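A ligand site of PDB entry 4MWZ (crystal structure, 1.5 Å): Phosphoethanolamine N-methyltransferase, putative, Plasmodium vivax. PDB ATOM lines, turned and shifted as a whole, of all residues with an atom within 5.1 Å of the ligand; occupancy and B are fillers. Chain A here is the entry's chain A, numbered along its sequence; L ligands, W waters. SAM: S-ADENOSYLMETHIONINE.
Water W3 lies within hydrogen-bond range of O of Asp 34 (2.7 Å) and O of the ligand (2.7 Å). Water W2 lies within hydrogen-bond range of an oxygen (OXT) of the ligand (2.8 Å), the side-chain hydroxyl (OG) of Ser 37 (3.2 Å) and the guanidinium group (NH1) of Arg 127 (3.3 Å). Water W4 bridges OD2 of Asp 61 (2.8 Å) and N of the ligand (2.9 Å).
OH of Tyr 19 lies close to SD of the ligand (3.2 Å). Merely in contact with the ligand: Asp 128 (3.2 Å), His 132 (3.4 Å), Cys 87 (3.7 Å), Lys 109 (3.7 Å), Gly 65 (3.8 Å), Tyr 35 (3.9 Å) and Leu 133 (3.99 Å). Hydrophobic or aromatic side chains that line the ligand: Tyr 19, Ile 36, Ile 86, Met 90, Ile 111, His 132 and Leu 133. 18 residues have an atom within 4 Å of the ligand: Tyr 19, Tyr 35, Ile 36, Ser 37, Gly 63, Gly 65, Asp 85, Ile 86, Cys 87, Met 90, Lys 109, Asp 110, Ile 111, Arg 127, Asp 128, Ser 129, His 132 and Leu 133. The nearest printed residue that does not touch the ligand is Val 84 (4.1 Å).
OXT of the ligand is in hydrogen-bond range of OG of Ser 37 (2.5 Å). An oxygen (O2') of the ligand sits at hydrogen-bond distance from the side-chain carboxylate (OD1) of Asp 85 (2.6 Å). O of Gly 63 sits at hydrogen-bond distance from N of the ligand (2.8 Å). OD1 of Asp 110 lies within hydrogen-bond range of N6 of the ligand (2.9 Å). N of Ile 36 lies within hydrogen-bond range of O of the ligand, at 2.9 Å. The side-chain sulfur of Met 90 lies within hydrogen-bond range of an oxygen (O3') of the ligand, 3.0 Å away. N of Ile 111 sits at hydrogen-bond distance from N1 of the ligand (3.0 Å). N of the ligand sits at hydrogen-bond distance from O of Arg 127 (3.1 Å). The side-chain hydroxyl (OG) of Ser 129 lies close to an oxygen (O4') of the ligand (3.4 Å). N3 of the ligand sits at hydrogen-bond distance from N of Ile 86 (3.3 Å).
OD1 of Asp 85 is in hydrogen-bond range of N of Cys 87 (2.9 Å). The backbone carbonyl oxygen (O) of Asp 85 lies within hydrogen-bond range of the backbone NH (N) of Lys 109, at 3.0 Å. OD2 of Asp 85 sits at hydrogen-bond distance from N of Gly 65 (2.8 Å). The side-chain carboxylate of Asp 85 is in hydrogen-bond range of the backbone NH of Ser 64. N of Gly 63 sits at hydrogen-bond distance from O of Val 84 (2.8 Å). The side-chain carboxylate of Asp 110 is in hydrogen-bond range of the backbone NH of Leu 112 (2.9 Å). The side-chain sulfur of Cys 87 lies close to the backbone NH of Met 90, 3.7 Å away. The backbone carbonyl oxygen of Arg 127 is in hydrogen-bond range of the side-chain hydroxyl of Ser 129 (3.0 Å).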
ATOM      1  N   GLN A  18       2.723  10.775  -4.850  1.00  0.00           N
ATOM      2  CA  GLN A  18       1.696  10.340  -3.915  1.00  0.00           C
ATOM      3  C   GLN A  18       0.970  11.482  -3.203  1.00  0.00           C
ATOM      4  O   GLN A  18      -0.254  11.498  -3.102  1.00  0.00           O
ATOM      5  CB  GLN A  18       2.362   9.430  -2.884  1.00  0.00           C
ATOM      6  CG  GLN A  18       1.490   9.056  -1.735  1.00  0.00           C
ATOM      7  CD  GLN A  18       2.088   7.917  -0.936  1.00  0.00           C
ATOM      8  OE1 GLN A  18       3.316   7.796  -0.815  1.00  0.00           O
ATOM      9  NE2 GLN A  18       1.219   7.082  -0.388  1.00  0.00           N
ATOM     10  N   TYR A  19       1.734  12.454  -2.710  1.00  0.00           N
ATOM     11  CA  TYR A  19       1.113  13.542  -1.970  1.00  0.00           C
ATOM     12  C   TYR A  19       1.050  14.809  -2.795  1.00  0.00           C
ATOM     13  O   TYR A  19       1.236  15.919  -2.264  1.00  0.00           O
ATOM     14  CB  TYR A  19       1.838  13.760  -0.634  1.00  0.00           C
ATOM     15  CG  TYR A  19       1.944  12.491   0.181  1.00  0.00           C
ATOM     16  CD1 TYR A  19       0.808  11.823   0.613  1.00  0.00           C
ATOM     17  CD2 TYR A  19       3.188  11.966   0.516  1.00  0.00           C
ATOM     18  CE1 TYR A  19       0.896  10.665   1.369  1.00  0.00           C
ATOM     19  CE2 TYR A  19       3.287  10.803   1.260  1.00  0.00           C
ATOM     20  CZ  TYR A  19       2.140  10.159   1.678  1.00  0.00           C
ATOM     21  OH  TYR A  19       2.245   9.017   2.427  1.00  0.00           O
ATOM     22  N   ASP A  34      -9.952  13.697   7.252  1.00  0.00           N
ATOM     23  CA  ASP A  34      -8.836  13.784   8.205  1.00  0.00           C
ATOM     24  C   ASP A  34      -7.838  12.637   8.100  1.00  0.00           C
ATOM     25  O   ASP A  34      -6.825  12.640   8.804  1.00  0.00           O
ATOM     26  CB  ASP A  34      -9.309  13.915   9.671  1.00  0.00           C
ATOM     27  CG  ASP A  34     -10.207  15.108   9.907  1.00  0.00           C
ATOM     28  OD1 ASP A  34      -9.891  16.202   9.414  1.00  0.00           O
ATOM     29  OD2 ASP A  34     -11.238  14.932  10.599  1.00  0.00           O
ATOM     30  N   TYR A  35      -8.115  11.669   7.237  1.00  0.00           N
ATOM     31  CA  TYR A  35      -7.250  10.498   7.116  1.00  0.00           C
ATOM     32  C   TYR A  35      -6.725  10.326   5.706  1.00  0.00           C
ATOM     33  O   TYR A  35      -7.439  10.579   4.718  1.00  0.00           O
ATOM     34  CB  TYR A  35      -7.993   9.229   7.532  1.00  0.00           C
ATOM     35  CG  TYR A  35      -8.307   9.192   8.995  1.00  0.00           C
ATOM     36  CD1 TYR A  35      -7.400   8.672   9.901  1.00  0.00           C
ATOM     37  CD2 TYR A  35      -9.506   9.710   9.484  1.00  0.00           C
ATOM     38  CE1 TYR A  35      -7.683   8.645  11.256  1.00  0.00           C
ATOM     39  CE2 TYR A  35      -9.796   9.692  10.830  1.00  0.00           C
ATOM     40  CZ  TYR A  35      -8.887   9.158  11.702  1.00  0.00           C
ATOM     41  OH  TYR A  35      -9.189   9.138  13.055  1.00  0.00           O
ATOM     42  N   ILE A  36      -5.473   9.871   5.609  1.00  0.00           N
ATOM     43  CA  ILE A  36      -4.870   9.511   4.329  1.00  0.00           C
ATOM     44  C   ILE A  36      -4.153   8.170   4.454  1.00  0.00           C
ATOM     45  O   ILE A  36      -3.146   7.918   3.781  1.00  0.00           O
ATOM     46  CB  ILE A  36      -3.932  10.621   3.767  1.00  0.00           C
ATOM     47  CG1 ILE A  36      -2.774  10.936   4.725  1.00  0.00           C
ATOM     48  CG2 ILE A  36      -4.738  11.890   3.457  1.00  0.00           C
ATOM     49  CD1 ILE A  36      -1.756  11.916   4.131  1.00  0.00           C
ATOM     50  N   SER A  37      -4.678   7.298   5.297  1.00  0.00           N
ATOM     51  CA  SER A  37      -4.204   5.914   5.326  1.00  0.00           C
ATOM     52  C   SER A  37      -5.291   4.908   5.637  1.00  0.00           C
ATOM     53  O   SER A  37      -6.393   5.271   6.070  1.00  0.00           O
ATOM     54  CB  SER A  37      -3.055   5.723   6.319  1.00  0.00           C
ATOM     55  OG  SER A  37      -3.531   5.685   7.657  1.00  0.00           O
ATOM     56  N   ASP A  61       2.545  11.220  17.519  1.00  0.00           N
ATOM     57  CA  ASP A  61       2.091  10.594  16.264  1.00  0.00           C
ATOM     58  C   ASP A  61       3.133  10.876  15.193  1.00  0.00           C
ATOM     59  O   ASP A  61       3.325  12.027  14.792  1.00  0.00           O
ATOM     60  CB  ASP A  61       0.724  11.157  15.845  1.00  0.00           C
ATOM     61  CG  ASP A  61       0.154  10.496  14.585  1.00  0.00           C
ATOM     62  OD1 ASP A  61       0.885   9.749  13.902  1.00  0.00           O
ATOM     63  OD2 ASP A  61      -1.035  10.740  14.272  1.00  0.00           O
ATOM     64  N   ILE A  62       3.837   9.833  14.743  1.00  0.00           N
ATOM     65  CA  ILE A  62       4.876   9.975  13.740  1.00  0.00           C
ATOM     66  C   ILE A  62       4.280   9.832  12.353  1.00  0.00           C
ATOM     67  O   ILE A  62       3.832   8.736  11.959  1.00  0.00           O
ATOM     68  CB  ILE A  62       5.986   8.932  13.939  1.00  0.00           C
ATOM     69  CG1 ILE A  62       6.623   9.105  15.325  1.00  0.00           C
ATOM     70  CG2 ILE A  62       7.033   9.048  12.834  1.00  0.00           C
ATOM     71  CD1 ILE A  62       7.690   8.057  15.643  1.00  0.00           C
ATOM     72  N   GLY A  63       4.249  10.943  11.611  1.00  0.00           N
ATOM     73  CA  GLY A  63       3.579  10.983  10.320  1.00  0.00           C
ATOM     74  C   GLY A  63       2.130  11.408  10.460  1.00  0.00           C
ATOM     75  O   GLY A  63       1.234  10.762   9.922  1.00  0.00           O
ATOM     76  N   SER A  64       1.896  12.522  11.163  1.00  0.00           N
ATOM     77  CA  SER A  64       0.546  12.843  11.600  1.00  0.00           C
ATOM     78  C   SER A  64      -0.419  13.277  10.487  1.00  0.00           C
ATOM     79  O   SER A  64      -1.626  13.344  10.718  1.00  0.00           O
ATOM     80  CB  SER A  64       0.602  13.880  12.716  1.00  0.00           C
ATOM     81  OG  SER A  64       1.409  14.974  12.346  1.00  0.00           O
ATOM     82  N   GLY A  65       0.100  13.555   9.291  1.00  0.00           N
ATOM     83  CA  GLY A  65      -0.769  13.807   8.142  1.00  0.00           C
ATOM     84  C   GLY A  65      -1.706  14.980   8.313  1.00  0.00           C
ATOM     85  O   GLY A  65      -1.281  16.060   8.687  1.00  0.00           O
ATOM     86  N   VAL A  84       3.984  14.890  14.385  1.00  0.00           N
ATOM     87  CA  VAL A  84       5.077  15.356  13.560  1.00  0.00           C
ATOM     88  C   VAL A  84       4.870  14.856  12.141  1.00  0.00           C
ATOM     89  O   VAL A  84       4.618  13.674  11.942  1.00  0.00           O
ATOM     90  CB  VAL A  84       6.428  14.858  14.066  1.00  0.00           C
ATOM     91  CG1 VAL A  84       7.537  15.317  13.129  1.00  0.00           C
ATOM     92  CG2 VAL A  84       6.684  15.349  15.484  1.00  0.00           C
ATOM     93  N   ASP A  85       4.951  15.732  11.158  1.00  0.00           N
ATOM     94  CA  ASP A  85       4.914  15.276   9.771  1.00  0.00           C
ATOM     95  C   ASP A  85       5.898  16.107   8.961  1.00  0.00           C
ATOM     96  O   ASP A  85       6.035  17.311   9.195  1.00  0.00           O
ATOM     97  CB  ASP A  85       3.500  15.396   9.161  1.00  0.00           C
ATOM     98  CG  ASP A  85       3.324  14.498   7.942  1.00  0.00           C
ATOM     99  OD1 ASP A  85       3.917  14.817   6.890  1.00  0.00           O
ATOM    100  OD2 ASP A  85       2.627  13.468   8.030  1.00  0.00           O
ATOM    101  N   ILE A  86       6.572  15.478   8.020  1.00  0.00           N
ATOM    102  CA  ILE A  86       7.573  16.169   7.223  1.00  0.00           C
ATOM    103  C   ILE A  86       6.929  17.118   6.201  1.00  0.00           C
ATOM    104  O   ILE A  86       7.593  18.029   5.691  1.00  0.00           O
ATOM    105  CB  ILE A  86       8.472  15.152   6.484  1.00  0.00           C
ATOM    106  CG1 ILE A  86       9.769  15.794   5.995  1.00  0.00           C
ATOM    107  CG2 ILE A  86       7.704  14.472   5.352  1.00  0.00           C
ATOM    108  CD1 ILE A  86      10.780  14.797   5.453  1.00  0.00           C
ATOM    109  N   CYS A  87       5.647  16.924   5.923  1.00  0.00           N
ATOM    110  CA  CYS A  87       4.962  17.713   4.905  1.00  0.00           C
ATOM    111  C   CYS A  87       4.304  18.954   5.519  1.00  0.00           C
ATOM    112  O   CYS A  87       3.256  18.860   6.157  1.00  0.00           O
ATOM    113  CB  CYS A  87       3.927  16.848   4.190  1.00  0.00           C
ATOM    114  SG  CYS A  87       3.006  17.694   2.906  1.00  0.00           S
ATOM    115  N   MET A  90       0.544  19.636   4.952  1.00  0.00           N
ATOM    116  CA  MET A  90      -0.369  18.823   5.751  1.00  0.00           C
ATOM    117  C   MET A  90      -0.439  19.360   7.177  1.00  0.00           C
ATOM    118  O   MET A  90      -1.504  19.396   7.783  1.00  0.00           O
ATOM    119  CB  MET A  90       0.100  17.369   5.807  1.00  0.00           C
ATOM    120  CG  MET A  90      -0.021  16.629   4.500  1.00  0.00           C
ATOM    121  SD  MET A  90       0.641  14.976   4.735  1.00  0.00           S
ATOM    122  CE  MET A  90       0.738  14.420   3.041  1.00  0.00           C
ATOM    123  N   LYS A 109       8.347  18.666  10.538  1.00  0.00           N
ATOM    124  CA  LYS A 109       9.739  18.259  10.591  1.00  0.00           C
ATOM    125  C   LYS A 109       9.894  16.805  10.159  1.00  0.00           C
ATOM    126  O   LYS A 109       8.958  16.005  10.274  1.00  0.00           O
ATOM    127  CB  LYS A 109      10.322  18.439  11.999  1.00  0.00           C
ATOM    128  CG  LYS A 109      11.832  18.701  11.992  1.00  0.00           C
ATOM    129  CD  LYS A 109      12.318  19.343  13.283  1.00  0.00           C
ATOM    130  CE  LYS A 109      13.831  19.541  13.259  1.00  0.00           C
ATOM    131  NZ  LYS A 109      14.358  19.914  14.611  1.00  0.00           N
ATOM    132  N   ASP A 110      11.068  16.486   9.631  1.00  0.00           N
ATOM    133  CA  ASP A 110      11.480  15.108   9.400  1.00  0.00           C
ATOM    134  C   ASP A 110      11.674  14.497  10.782  1.00  0.00           C
ATOM    135  O   ASP A 110      12.430  15.042  11.592  1.00  0.00           O
ATOM    136  CB  ASP A 110      12.803  15.124   8.623  1.00  0.00           C
ATOM    137  CG  ASP A 110      13.327  13.746   8.295  1.00  0.00           C
ATOM    138  OD1 ASP A 110      12.826  12.730   8.835  1.00  0.00           O
ATOM    139  OD2 ASP A 110      14.287  13.679   7.489  1.00  0.00           O
ATOM    140  N   ILE A 111      10.992  13.386  11.075  1.00  0.00           N
ATOM    141  CA  ILE A 111      11.081  12.780  12.395  1.00  0.00           C
ATOM    142  C   ILE A 111      12.524  12.363  12.701  1.00  0.00           C
ATOM    143  O   ILE A 111      12.945  12.373  13.856  1.00  0.00           O
ATOM    144  CB  ILE A 111      10.100  11.583  12.528  1.00  0.00           C
ATOM    145  CG1 ILE A 111       9.983  11.137  13.992  1.00  0.00           C
ATOM    146  CG2 ILE A 111      10.516  10.435  11.618  1.00  0.00           C
ATOM    147  CD1 ILE A 111       9.387  12.216  14.888  1.00  0.00           C
ATOM    148  N   LEU A 112      13.291  12.071  11.656  1.00  0.00           N
ATOM    149  CA  LEU A 112      14.689  11.682  11.837  1.00  0.00           C
ATOM    150  C   LEU A 112      15.538  12.832  12.357  1.00  0.00           C
ATOM    151  O   LEU A 112      16.623  12.613  12.900  1.00  0.00           O
ATOM    152  CB  LEU A 112      15.253  11.177  10.507  1.00  0.00           C
ATOM    153  CG  LEU A 112      14.597   9.899   9.987  1.00  0.00           C
ATOM    154  CD1 LEU A 112      15.067   9.588   8.575  1.00  0.00           C
ATOM    155  CD2 LEU A 112      14.893   8.748  10.916  1.00  0.00           C
ATOM    156  N   ARG A 127       1.002   5.417  11.863  1.00  0.00           N
ATOM    157  CA  ARG A 127       0.111   4.701  10.962  1.00  0.00           C
ATOM    158  C   ARG A 127       0.545   4.889   9.520  1.00  0.00           C
ATOM    159  O   ARG A 127       0.427   5.987   8.952  1.00  0.00           O
ATOM    160  CB  ARG A 127      -1.324   5.167  11.161  1.00  0.00           C
ATOM    161  CG  ARG A 127      -1.841   5.033  12.570  1.00  0.00           C
ATOM    162  CD  ARG A 127      -2.119   3.578  12.961  1.00  0.00           C
ATOM    163  NE  ARG A 127      -2.931   2.944  11.931  1.00  0.00           N
ATOM    164  CZ  ARG A 127      -4.249   3.147  11.807  1.00  0.00           C
ATOM    165  NH1 ARG A 127      -4.915   3.900  12.683  1.00  0.00           N
ATOM    166  NH2 ARG A 127      -4.904   2.563  10.820  1.00  0.00           N
ATOM    167  N   ASP A 128       1.025   3.805   8.931  1.00  0.00           N
ATOM    168  CA  ASP A 128       1.441   3.755   7.524  1.00  0.00           C
ATOM    169  C   ASP A 128       2.308   4.920   7.111  1.00  0.00           C
ATOM    170  O   ASP A 128       2.047   5.579   6.102  1.00  0.00           O
ATOM    171  CB  ASP A 128       0.228   3.605   6.580  1.00  0.00           C
ATOM    172  CG  ASP A 128      -0.611   2.376   6.885  1.00  0.00           C
ATOM    173  OD1 ASP A 128      -0.220   1.541   7.722  1.00  0.00           O
ATOM    174  OD2 ASP A 128      -1.699   2.255   6.274  1.00  0.00           O
ATOM    175  N   SER A 129       3.354   5.166   7.904  1.00  0.00           N
ATOM    176  CA  SER A 129       4.273   6.266   7.631  1.00  0.00           C
ATOM    177  C   SER A 129       5.727   5.810   7.598  1.00  0.00           C
ATOM    178  O   SER A 129       6.545   6.424   6.920  1.00  0.00           O
ATOM    179  CB  SER A 129       4.121   7.351   8.688  1.00  0.00           C
ATOM    180  OG  SER A 129       2.786   7.869   8.707  1.00  0.00           O
ATOM    181  N   HIS A 132       8.085   5.026   4.497  1.00  0.00           N
ATOM    182  CA  HIS A 132       8.811   6.037   3.736  1.00  0.00           C
ATOM    183  C   HIS A 132      10.295   6.025   4.066  1.00  0.00           C
ATOM    184  O   HIS A 132      11.084   6.680   3.392  1.00  0.00           O
ATOM    185  CB  HIS A 132       8.231   7.413   4.016  1.00  0.00           C
ATOM    186  CG  HIS A 132       6.905   7.656   3.371  1.00  0.00           C
ATOM    187  ND1 HIS A 132       6.738   7.632   1.999  1.00  0.00           N
ATOM    188  CD2 HIS A 132       5.681   7.915   3.890  1.00  0.00           C
ATOM    189  CE1 HIS A 132       5.471   7.876   1.707  1.00  0.00           C
ATOM    190  NE2 HIS A 132       4.815   8.059   2.834  1.00  0.00           N
ATOM    191  N   LEU A 133      10.670   5.271   5.104  1.00  0.00           N
ATOM    192  CA  LEU A 133      12.041   5.293   5.603  1.00  0.00           C
ATOM    193  C   LEU A 133      12.816   4.084   5.118  1.00  0.00           C
ATOM    194  O   LEU A 133      12.277   2.978   5.063  1.00  0.00           O
ATOM    195  CB  LEU A 133      12.051   5.304   7.134  1.00  0.00           C
ATOM    196  CG  LEU A 133      11.806   6.630   7.863  1.00  0.00           C
ATOM    197  CD1 LEU A 133      10.620   7.431   7.332  1.00  0.00           C
ATOM    198  CD2 LEU A 133      11.664   6.388   9.366  1.00  0.00           C
HETATM  199  N   SAM L   1      -0.697   8.766   9.734  1.00  0.00           N
HETATM  200  CA  SAM L   1      -1.421   9.602   8.782  1.00  0.00           C
HETATM  201  C   SAM L   1      -2.721   8.920   8.433  1.00  0.00           C
HETATM  202  O   SAM L   1      -3.569   9.526   7.786  1.00  0.00           O
HETATM  203  OXT SAM L   1      -2.930   7.772   8.817  1.00  0.00           O
HETATM  204  CB  SAM L   1      -0.621   9.825   7.516  1.00  0.00           C
HETATM  205  CG  SAM L   1      -0.397   8.571   6.664  1.00  0.00           C
HETATM  206  SD  SAM L   1       0.505   8.957   5.155  1.00  0.00           S
HETATM  207  CE  SAM L   1       0.286   7.416   4.230  1.00  0.00           C
HETATM  208  C5' SAM L   1       2.231   8.838   5.681  1.00  0.00           C
HETATM  209  C4' SAM L   1       2.738  10.182   6.202  1.00  0.00           C
HETATM  210  O4' SAM L   1       4.118  10.038   6.517  1.00  0.00           O
HETATM  211  C3' SAM L   1       2.654  11.325   5.196  1.00  0.00           C
HETATM  212  O3' SAM L   1       1.798  12.371   5.666  1.00  0.00           O
HETATM  213  C2' SAM L   1       4.096  11.812   5.075  1.00  0.00           C
HETATM  214  O2' SAM L   1       4.262  13.205   4.916  1.00  0.00           O
HETATM  215  C1' SAM L   1       4.682  11.328   6.389  1.00  0.00           C
HETATM  216  N9  SAM L   1       6.151  11.205   6.398  1.00  0.00           N
HETATM  217  C8  SAM L   1       6.937  10.647   5.433  1.00  0.00           C
HETATM  218  N7  SAM L   1       8.227  10.727   5.827  1.00  0.00           N
HETATM  219  C5  SAM L   1       8.268  11.338   7.042  1.00  0.00           C
HETATM  220  C6  SAM L   1       9.322  11.674   7.899  1.00  0.00           C
HETATM  221  N6  SAM L   1      10.595  11.416   7.601  1.00  0.00           N
HETATM  222  N1  SAM L   1       9.011  12.296   9.075  1.00  0.00           N
HETATM  223  C2  SAM L   1       7.709  12.586   9.421  1.00  0.00           C
HETATM  224  N3  SAM L   1       6.677  12.260   8.579  1.00  0.00           N
HETATM  225  C4  SAM L   1       6.962  11.626   7.409  1.00  0.00           C
HETATM  226  O   HOH W   1       6.744  11.221   2.012  1.00  0.00           O
HETATM  227  O   HOH W   2      -4.643   6.489  10.588  1.00  0.00           O
HETATM  228  O   HOH W   3      -4.185  12.120   8.408  1.00  0.00           O
HETATM  229  O   HOH W   4      -2.148   9.230  12.179  1.00  0.00           O
HETATM  230  O   HOH W   5       1.063   8.234  11.843  1.00  0.00           O
HETATM  231  O   HOH W   6       5.758  13.529   2.642  1.00  0.00           O
HETATM  232  O   HOH W   7      -4.215  10.725  10.858  1.00  0.00           O
HETATM  233  O   HOH W   8       9.672  11.005   3.122  1.00  0.00           O
